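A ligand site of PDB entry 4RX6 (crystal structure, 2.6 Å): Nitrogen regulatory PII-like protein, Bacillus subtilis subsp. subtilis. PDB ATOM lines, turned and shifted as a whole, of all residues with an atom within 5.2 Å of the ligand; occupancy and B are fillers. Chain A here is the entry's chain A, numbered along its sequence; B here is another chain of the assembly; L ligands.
An oxygen (O2) of the ligand lies within salt-bridge range of the side-chain amino group of Lys 99 (2.7 Å). O1 of the ligand lies within hydrogen-bond range of OG1 of Thr 35 of chain B, 2.8 Å away. N of Gly 96 sits at hydrogen-bond distance from O8 of the ligand. The side-chain hydroxyl of Thr 38 of chain B lies within hydrogen-bond range of a nitrogen (N5) of the ligand, at 2.8 Å. The backbone NH of Val 73 of chain B sits at hydrogen-bond distance from a nitrogen (N4) of the ligand. A nitrogen (N3) of the ligand sits at hydrogen-bond distance from the backbone carbonyl oxygen (O) of Val 73 of chain B (2.9 Å). O8 of the ligand is in hydrogen-bond range of N of Gly 98, 3.3 Å away. The side-chain hydroxyl (OG) of Ser 36 of chain B sits at hydrogen-bond distance from a nitrogen (N2) of the ligand (3.0 Å). The guanidinium group (NH1) of Arg 67 lies close to an oxygen (O12) of the ligand (3.3 Å).
The backbone NH (N) of Lys 99 sits at hydrogen-bond distance from the backbone carbonyl oxygen (O) of Val 16 (3.0 Å). N of Glu 71 of chain B is in hydrogen-bond range of O of Thr 38 of chain B (2.8 Å). O of Gly 44 lies within hydrogen-bond range of N of Tyr 65. The backbone carbonyl oxygen of Leu 37 of chain B lies within hydrogen-bond range of the backbone NH of Cys 45 (2.8 Å). The backbone carbonyl oxygen (O) of Asp 97 lies within hydrogen-bond range of the side-chain hydroxyl (OG1) of Thr 17 (2.9 Å).
Val 16 touches the ligand (CG1 to O11, 3.5 Å). Gly 44 touches the ligand. CB of Pro 95 touches O5 of the ligand (3.7 Å). Asp 97 touches the ligand (N to O8, 3.6 Å). Leu 37 of chain B touches the ligand. Glu 71 of chain B touches the ligand (O to C9, 3.1 Å). Ile 72 of chain B touches the ligand (C to N4, 3.8 Å). CD2 of Leu 121 of chain B touches N3 of the ligand, 3.98 Å away. Hydrophobic or aromatic side chains within 4 Å of the ligand: Val 16, Pro 95, Val 73 of chain B and Leu 121 of chain B. The nearest printed residue that does not touch the ligand is Cys 45 (4.01 Å).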
ATOM      1  N   VAL A  16     -16.245   1.787  11.359  1.00  0.00           N
ATOM      2  CA  VAL A  16     -17.148   1.488  12.462  1.00  0.00           C
ATOM      3  C   VAL A  16     -16.968   0.034  12.913  1.00  0.00           C
ATOM      4  O   VAL A  16     -17.036  -0.886  12.082  1.00  0.00           O
ATOM      5  CB  VAL A  16     -18.595   1.713  12.057  1.00  0.00           C
ATOM      6  CG1 VAL A  16     -19.478   1.637  13.298  1.00  0.00           C
ATOM      7  CG2 VAL A  16     -18.736   3.035  11.348  1.00  0.00           C
ATOM      8  N   THR A  17     -16.737  -0.173  14.211  1.00  0.00           N
ATOM      9  CA  THR A  17     -16.234  -1.462  14.688  1.00  0.00           C
ATOM     10  C   THR A  17     -16.526  -1.689  16.161  1.00  0.00           C
ATOM     11  O   THR A  17     -17.188  -0.893  16.809  1.00  0.00           O
ATOM     12  CB  THR A  17     -14.695  -1.564  14.446  1.00  0.00           C
ATOM     13  OG1 THR A  17     -14.218  -2.875  14.782  1.00  0.00           O
ATOM     14  CG2 THR A  17     -13.941  -0.545  15.261  1.00  0.00           C
ATOM     15  N   HIS A  43     -23.515   3.754  18.226  1.00  0.00           N
ATOM     16  CA  HIS A  43     -24.161   2.461  18.413  1.00  0.00           C
ATOM     17  C   HIS A  43     -24.394   1.826  17.056  1.00  0.00           C
ATOM     18  O   HIS A  43     -24.546   2.518  16.064  1.00  0.00           O
ATOM     19  CB  HIS A  43     -25.492   2.607  19.152  1.00  0.00           C
ATOM     20  CG  HIS A  43     -25.371   3.175  20.530  1.00  0.00           C
ATOM     21  ND1 HIS A  43     -25.168   2.397  21.648  1.00  0.00           N
ATOM     22  CD2 HIS A  43     -25.444   4.456  20.970  1.00  0.00           C
ATOM     23  CE1 HIS A  43     -25.109   3.170  22.713  1.00  0.00           C
ATOM     24  NE2 HIS A  43     -25.268   4.427  22.331  1.00  0.00           N
ATOM     25  N   GLY A  44     -24.418   0.505  16.989  1.00  0.00           N
ATOM     26  CA  GLY A  44     -24.695  -0.181  15.748  1.00  0.00           C
ATOM     27  C   GLY A  44     -26.044  -0.818  15.909  1.00  0.00           C
ATOM     28  O   GLY A  44     -26.460  -1.077  17.024  1.00  0.00           O
ATOM     29  N   CYS A  45     -26.727  -1.074  14.804  1.00  0.00           N
ATOM     30  CA  CYS A  45     -28.026  -1.726  14.844  1.00  0.00           C
ATOM     31  C   CYS A  45     -28.028  -2.859  13.822  1.00  0.00           C
ATOM     32  O   CYS A  45     -27.545  -2.685  12.704  1.00  0.00           O
ATOM     33  CB  CYS A  45     -29.170  -0.730  14.571  1.00  0.00           C
ATOM     34  SG  CYS A  45     -30.790  -1.201  15.283  1.00  0.00           S
ATOM     35  N   GLY A  46     -28.524  -4.017  14.225  1.00  0.00           N
ATOM     36  CA  GLY A  46     -28.565  -5.176  13.354  1.00  0.00           C
ATOM     37  C   GLY A  46     -29.992  -5.534  13.027  1.00  0.00           C
ATOM     38  O   GLY A  46     -30.850  -5.622  13.902  1.00  0.00           O
ATOM     39  N   TYR A  65     -26.057  -2.624  19.398  1.00  0.00           N
ATOM     40  CA  TYR A  65     -24.719  -2.804  19.957  1.00  0.00           C
ATOM     41  C   TYR A  65     -24.034  -1.494  20.277  1.00  0.00           C
ATOM     42  O   TYR A  65     -24.431  -0.433  19.793  1.00  0.00           O
ATOM     43  CB  TYR A  65     -23.832  -3.577  18.985  1.00  0.00           C
ATOM     44  CG  TYR A  65     -24.494  -4.784  18.384  1.00  0.00           C
ATOM     45  CD1 TYR A  65     -24.473  -6.016  19.042  1.00  0.00           C
ATOM     46  CD2 TYR A  65     -25.148  -4.710  17.161  1.00  0.00           C
ATOM     47  CE1 TYR A  65     -25.092  -7.129  18.495  1.00  0.00           C
ATOM     48  CE2 TYR A  65     -25.759  -5.810  16.606  1.00  0.00           C
ATOM     49  CZ  TYR A  65     -25.739  -7.028  17.275  1.00  0.00           C
ATOM     50  OH  TYR A  65     -26.351  -8.125  16.695  1.00  0.00           O
ATOM     51  N   ARG A  67     -20.811   0.417  19.377  1.00  0.00           N
ATOM     52  CA  ARG A  67     -19.718   0.359  18.427  1.00  0.00           C
ATOM     53  C   ARG A  67     -18.897   1.619  18.574  1.00  0.00           C
ATOM     54  O   ARG A  67     -19.321   2.595  19.199  1.00  0.00           O
ATOM     55  CB  ARG A  67     -20.222   0.220  17.002  1.00  0.00           C
ATOM     56  CG  ARG A  67     -21.340  -0.794  16.832  1.00  0.00           C
ATOM     57  CD  ARG A  67     -20.877  -2.088  16.189  1.00  0.00           C
ATOM     58  NE  ARG A  67     -20.509  -3.111  17.162  1.00  0.00           N
ATOM     59  CZ  ARG A  67     -20.990  -4.350  17.174  1.00  0.00           C
ATOM     60  NH1 ARG A  67     -21.849  -4.761  16.265  1.00  0.00           N
ATOM     61  NH2 ARG A  67     -20.576  -5.191  18.117  1.00  0.00           N
ATOM     62  N   PRO A  95     -18.503 -11.678  14.152  1.00  0.00           N
ATOM     63  CA  PRO A  95     -19.267 -10.530  13.672  1.00  0.00           C
ATOM     64  C   PRO A  95     -19.159  -9.383  14.697  1.00  0.00           C
ATOM     65  O   PRO A  95     -19.055  -9.641  15.903  1.00  0.00           O
ATOM     66  CB  PRO A  95     -20.673 -11.113  13.613  1.00  0.00           C
ATOM     67  CG  PRO A  95     -20.727 -11.890  14.918  1.00  0.00           C
ATOM     68  CD  PRO A  95     -19.320 -12.517  15.046  1.00  0.00           C
ATOM     69  N   GLY A  96     -19.167  -8.141  14.196  1.00  0.00           N
ATOM     70  CA  GLY A  96     -18.847  -6.962  14.983  1.00  0.00           C
ATOM     71  C   GLY A  96     -17.423  -6.519  14.714  1.00  0.00           C
ATOM     72  O   GLY A  96     -16.875  -5.658  15.397  1.00  0.00           O
ATOM     73  N   ASP A  97     -16.802  -7.126  13.708  1.00  0.00           N
ATOM     74  CA  ASP A  97     -15.505  -6.678  13.239  1.00  0.00           C
ATOM     75  C   ASP A  97     -15.702  -5.336  12.565  1.00  0.00           C
ATOM     76  O   ASP A  97     -14.771  -4.529  12.455  1.00  0.00           O
ATOM     77  CB  ASP A  97     -14.949  -7.655  12.204  1.00  0.00           C
ATOM     78  CG  ASP A  97     -14.116  -8.769  12.803  1.00  0.00           C
ATOM     79  OD1 ASP A  97     -13.612  -8.629  13.939  1.00  0.00           O
ATOM     80  OD2 ASP A  97     -13.945  -9.782  12.092  1.00  0.00           O
ATOM     81  N   GLY A  98     -16.919  -5.107  12.062  1.00  0.00           N
ATOM     82  CA  GLY A  98     -17.259  -3.837  11.472  1.00  0.00           C
ATOM     83  C   GLY A  98     -16.689  -3.593  10.089  1.00  0.00           C
ATOM     84  O   GLY A  98     -15.954  -4.427   9.541  1.00  0.00           O
ATOM     85  N   LYS A  99     -17.022  -2.438   9.521  1.00  0.00           N
ATOM     86  CA  LYS A  99     -16.707  -2.161   8.139  1.00  0.00           C
ATOM     87  C   LYS A  99     -15.881  -0.920   8.037  1.00  0.00           C
ATOM     88  O   LYS A  99     -15.771  -0.174   9.016  1.00  0.00           O
ATOM     89  CB  LYS A  99     -18.001  -1.976   7.351  1.00  0.00           C
ATOM     90  CG  LYS A  99     -18.943  -3.142   7.533  1.00  0.00           C
ATOM     91  CD  LYS A  99     -19.507  -3.593   6.218  1.00  0.00           C
ATOM     92  CE  LYS A  99     -20.315  -4.861   6.391  1.00  0.00           C
ATOM     93  NZ  LYS A  99     -21.429  -4.700   7.335  1.00  0.00           N
ATOM     94  N   PHE A 101     -15.583   2.517   5.406  1.00  0.00           N
ATOM     95  CA  PHE A 101     -16.085   3.264   4.256  1.00  0.00           C
ATOM     96  C   PHE A 101     -15.103   4.331   3.848  1.00  0.00           C
ATOM     97  O   PHE A 101     -14.520   4.965   4.702  1.00  0.00           O
ATOM     98  CB  PHE A 101     -17.374   3.939   4.621  1.00  0.00           C
ATOM     99  CG  PHE A 101     -18.363   3.051   5.315  1.00  0.00           C
ATOM    100  CD1 PHE A 101     -19.092   2.125   4.613  1.00  0.00           C
ATOM    101  CD2 PHE A 101     -18.604   3.178   6.647  1.00  0.00           C
ATOM    102  CE1 PHE A 101     -20.002   1.354   5.242  1.00  0.00           C
ATOM    103  CE2 PHE A 101     -19.530   2.398   7.268  1.00  0.00           C
ATOM    104  CZ  PHE A 101     -20.223   1.491   6.573  1.00  0.00           C
ATOM    105  N   THR B  35     -29.539  -4.393   6.320  1.00  0.00           N
ATOM    106  CA  THR B  35     -29.055  -5.447   7.211  1.00  0.00           C
ATOM    107  C   THR B  35     -28.504  -4.858   8.510  1.00  0.00           C
ATOM    108  O   THR B  35     -28.549  -5.500   9.548  1.00  0.00           O
ATOM    109  CB  THR B  35     -27.982  -6.365   6.493  1.00  0.00           C
ATOM    110  OG1 THR B  35     -26.651  -6.009   6.880  1.00  0.00           O
ATOM    111  CG2 THR B  35     -28.105  -6.274   4.962  1.00  0.00           C
ATOM    112  N   SER B  36     -27.969  -3.644   8.450  1.00  0.00           N
ATOM    113  CA  SER B  36     -27.449  -2.999   9.648  1.00  0.00           C
ATOM    114  C   SER B  36     -27.167  -1.496   9.414  1.00  0.00           C
ATOM    115  O   SER B  36     -26.852  -1.077   8.301  1.00  0.00           O
ATOM    116  CB  SER B  36     -26.238  -3.762  10.201  1.00  0.00           C
ATOM    117  OG  SER B  36     -25.110  -3.565   9.395  1.00  0.00           O
ATOM    118  N   LEU B  37     -27.332  -0.704  10.464  1.00  0.00           N
ATOM    119  CA  LEU B  37     -27.125   0.731  10.375  1.00  0.00           C
ATOM    120  C   LEU B  37     -26.352   1.236  11.600  1.00  0.00           C
ATOM    121  O   LEU B  37     -26.098   0.478  12.527  1.00  0.00           O
ATOM    122  CB  LEU B  37     -28.485   1.414  10.214  1.00  0.00           C
ATOM    123  CG  LEU B  37     -29.611   1.152  11.210  1.00  0.00           C
ATOM    124  CD1 LEU B  37     -29.514   2.118  12.366  1.00  0.00           C
ATOM    125  CD2 LEU B  37     -30.963   1.317  10.551  1.00  0.00           C
ATOM    126  N   THR B  38     -25.948   2.506  11.576  1.00  0.00           N
ATOM    127  CA  THR B  38     -25.218   3.138  12.687  1.00  0.00           C
ATOM    128  C   THR B  38     -26.035   4.329  13.144  1.00  0.00           C
ATOM    129  O   THR B  38     -26.594   5.036  12.311  1.00  0.00           O
ATOM    130  CB  THR B  38     -23.812   3.647  12.254  1.00  0.00           C
ATOM    131  OG1 THR B  38     -23.037   2.581  11.708  1.00  0.00           O
ATOM    132  CG2 THR B  38     -23.047   4.248  13.433  1.00  0.00           C
ATOM    133  N   GLU B  71     -26.960   6.647  10.012  1.00  0.00           N
ATOM    134  CA  GLU B  71     -26.177   6.548   8.794  1.00  0.00           C
ATOM    135  C   GLU B  71     -26.294   5.142   8.228  1.00  0.00           C
ATOM    136  O   GLU B  71     -25.879   4.187   8.843  1.00  0.00           O
ATOM    137  CB  GLU B  71     -24.712   6.896   9.038  1.00  0.00           C
ATOM    138  CG  GLU B  71     -24.495   7.652  10.333  1.00  0.00           C
ATOM    139  CD  GLU B  71     -23.058   8.138  10.543  1.00  0.00           C
ATOM    140  OE1 GLU B  71     -22.694   8.341  11.722  1.00  0.00           O
ATOM    141  OE2 GLU B  71     -22.314   8.335   9.562  1.00  0.00           O
ATOM    142  N   ILE B  72     -26.905   5.021   7.052  1.00  0.00           N
ATOM    143  CA  ILE B  72     -26.981   3.740   6.387  1.00  0.00           C
ATOM    144  C   ILE B  72     -26.151   3.753   5.097  1.00  0.00           C
ATOM    145  O   ILE B  72     -26.273   4.681   4.305  1.00  0.00           O
ATOM    146  CB  ILE B  72     -28.430   3.429   6.023  1.00  0.00           C
ATOM    147  CG1 ILE B  72     -29.316   3.605   7.270  1.00  0.00           C
ATOM    148  CG2 ILE B  72     -28.523   2.023   5.459  1.00  0.00           C
ATOM    149  CD1 ILE B  72     -30.644   4.291   7.000  1.00  0.00           C
ATOM    150  N   VAL B  73     -25.297   2.754   4.904  1.00  0.00           N
ATOM    151  CA  VAL B  73     -24.521   2.628   3.683  1.00  0.00           C
ATOM    152  C   VAL B  73     -25.056   1.479   2.828  1.00  0.00           C
ATOM    153  O   VAL B  73     -25.126   0.345   3.278  1.00  0.00           O
ATOM    154  CB  VAL B  73     -23.037   2.405   3.971  1.00  0.00           C
ATOM    155  CG1 VAL B  73     -22.273   2.097   2.695  1.00  0.00           C
ATOM    156  CG2 VAL B  73     -22.453   3.625   4.654  1.00  0.00           C
ATOM    157  N   VAL B  74     -25.433   1.787   1.590  1.00  0.00           N
ATOM    158  CA  VAL B  74     -26.087   0.828   0.713  1.00  0.00           C
ATOM    159  C   VAL B  74     -25.453   0.817  -0.665  1.00  0.00           C
ATOM    160  O   VAL B  74     -24.801   1.770  -1.072  1.00  0.00           O
ATOM    161  CB  VAL B  74     -27.563   1.200   0.526  1.00  0.00           C
ATOM    162  CG1 VAL B  74     -28.248   1.236   1.874  1.00  0.00           C
ATOM    163  CG2 VAL B  74     -27.677   2.542  -0.157  1.00  0.00           C
ATOM    164  N   ASN B 110     -15.166  -5.082   4.084  1.00  0.00           N
ATOM    165  CA  ASN B 110     -15.638  -5.898   5.175  1.00  0.00           C
ATOM    166  C   ASN B 110     -14.421  -6.367   6.004  1.00  0.00           C
ATOM    167  O   ASN B 110     -13.539  -7.037   5.475  1.00  0.00           O
ATOM    168  CB  ASN B 110     -16.415  -7.084   4.622  1.00  0.00           C
ATOM    169  CG  ASN B 110     -17.305  -7.732   5.648  1.00  0.00           C
ATOM    170  OD1 ASN B 110     -16.830  -8.270   6.632  1.00  0.00           O
ATOM    171  ND2 ASN B 110     -18.614  -7.670   5.435  1.00  0.00           N
ATOM    172  N   LEU B 121     -20.932  -5.161   1.642  1.00  0.00           N
ATOM    173  CA  LEU B 121     -22.068  -4.683   2.430  1.00  0.00           C
ATOM    174  C   LEU B 121     -23.077  -5.792   2.743  1.00  0.00           C
ATOM    175  O   LEU B 121     -22.979  -6.899   2.203  1.00  0.00           O
ATOM    176  CB  LEU B 121     -22.762  -3.536   1.701  1.00  0.00           C
ATOM    177  CG  LEU B 121     -21.924  -2.254   1.603  1.00  0.00           C
ATOM    178  CD1 LEU B 121     -22.643  -1.185   0.772  1.00  0.00           C
ATOM    179  CD2 LEU B 121     -21.627  -1.729   2.991  1.00  0.00           C
ATOM    180  OXT LEU B 121     -23.997  -5.612   3.544  1.00  0.00           O
HETATM  181  P1  LIG L   1     -23.605  -7.491   8.216  1.00  0.00           P
HETATM  182  O1  LIG L   1     -24.996  -7.975   7.871  1.00  0.00           O
HETATM  183  O2  LIG L   1     -23.557  -5.988   8.390  1.00  0.00           O
HETATM  184  O3  LIG L   1     -22.482  -8.062   7.368  1.00  0.00           O
HETATM  185  P2  LIG L   1     -22.801  -7.209  10.936  1.00  0.00           P
HETATM  186  O4  LIG L   1     -23.954  -6.383  11.475  1.00  0.00           O
HETATM  187  O5  LIG L   1     -22.035  -8.138  11.855  1.00  0.00           O
HETATM  188  O6  LIG L   1     -23.296  -8.099   9.686  1.00  0.00           O
HETATM  189  P3  LIG L   1     -20.492  -5.552  11.085  1.00  0.00           P
HETATM  190  O7  LIG L   1     -19.576  -4.939  10.052  1.00  0.00           O
HETATM  191  O8  LIG L   1     -19.938  -6.484  12.113  1.00  0.00           O
HETATM  192  O9  LIG L   1     -21.750  -6.173  10.293  1.00  0.00           O
HETATM  193  O10 LIG L   1     -21.166  -4.340  11.877  1.00  0.00           O
HETATM  194  C1  LIG L   1     -20.309  -3.499  12.634  1.00  0.00           C
HETATM  195  C2  LIG L   1     -21.002  -2.178  12.855  1.00  0.00           C
HETATM  196  O11 LIG L   1     -20.648  -1.317  11.786  1.00  0.00           O
HETATM  197  C3  LIG L   1     -22.512  -2.274  12.789  1.00  0.00           C
HETATM  198  O12 LIG L   1     -23.121  -2.656  14.043  1.00  0.00           O
HETATM  199  C4  LIG L   1     -22.864  -0.872  12.382  1.00  0.00           C
HETATM  200  O13 LIG L   1     -22.744  -0.044  13.536  1.00  0.00           O
HETATM  201  C5  LIG L   1     -21.759  -0.496  11.414  1.00  0.00           C
HETATM  202  N1  LIG L   1     -22.250  -0.860  10.055  1.00  0.00           N
HETATM  203  C6  LIG L   1     -22.184  -2.072   9.479  1.00  0.00           C
HETATM  204  N2  LIG L   1     -22.767  -2.084   8.245  1.00  0.00           N
HETATM  205  C7  LIG L   1     -23.225  -0.842   8.027  1.00  0.00           C
HETATM  206  C8  LIG L   1     -23.938  -0.160   6.933  1.00  0.00           C
HETATM  207  N3  LIG L   1     -24.291  -0.814   5.797  1.00  0.00           N
HETATM  208  N4  LIG L   1     -24.223   1.156   7.100  1.00  0.00           N
HETATM  209  C9  LIG L   1     -23.889   1.831   8.224  1.00  0.00           C
HETATM  210  N5  LIG L   1     -23.246   1.271   9.260  1.00  0.00           N
HETATM  211  C10 LIG L   1     -22.880  -0.037   9.220  1.00  0.00           C
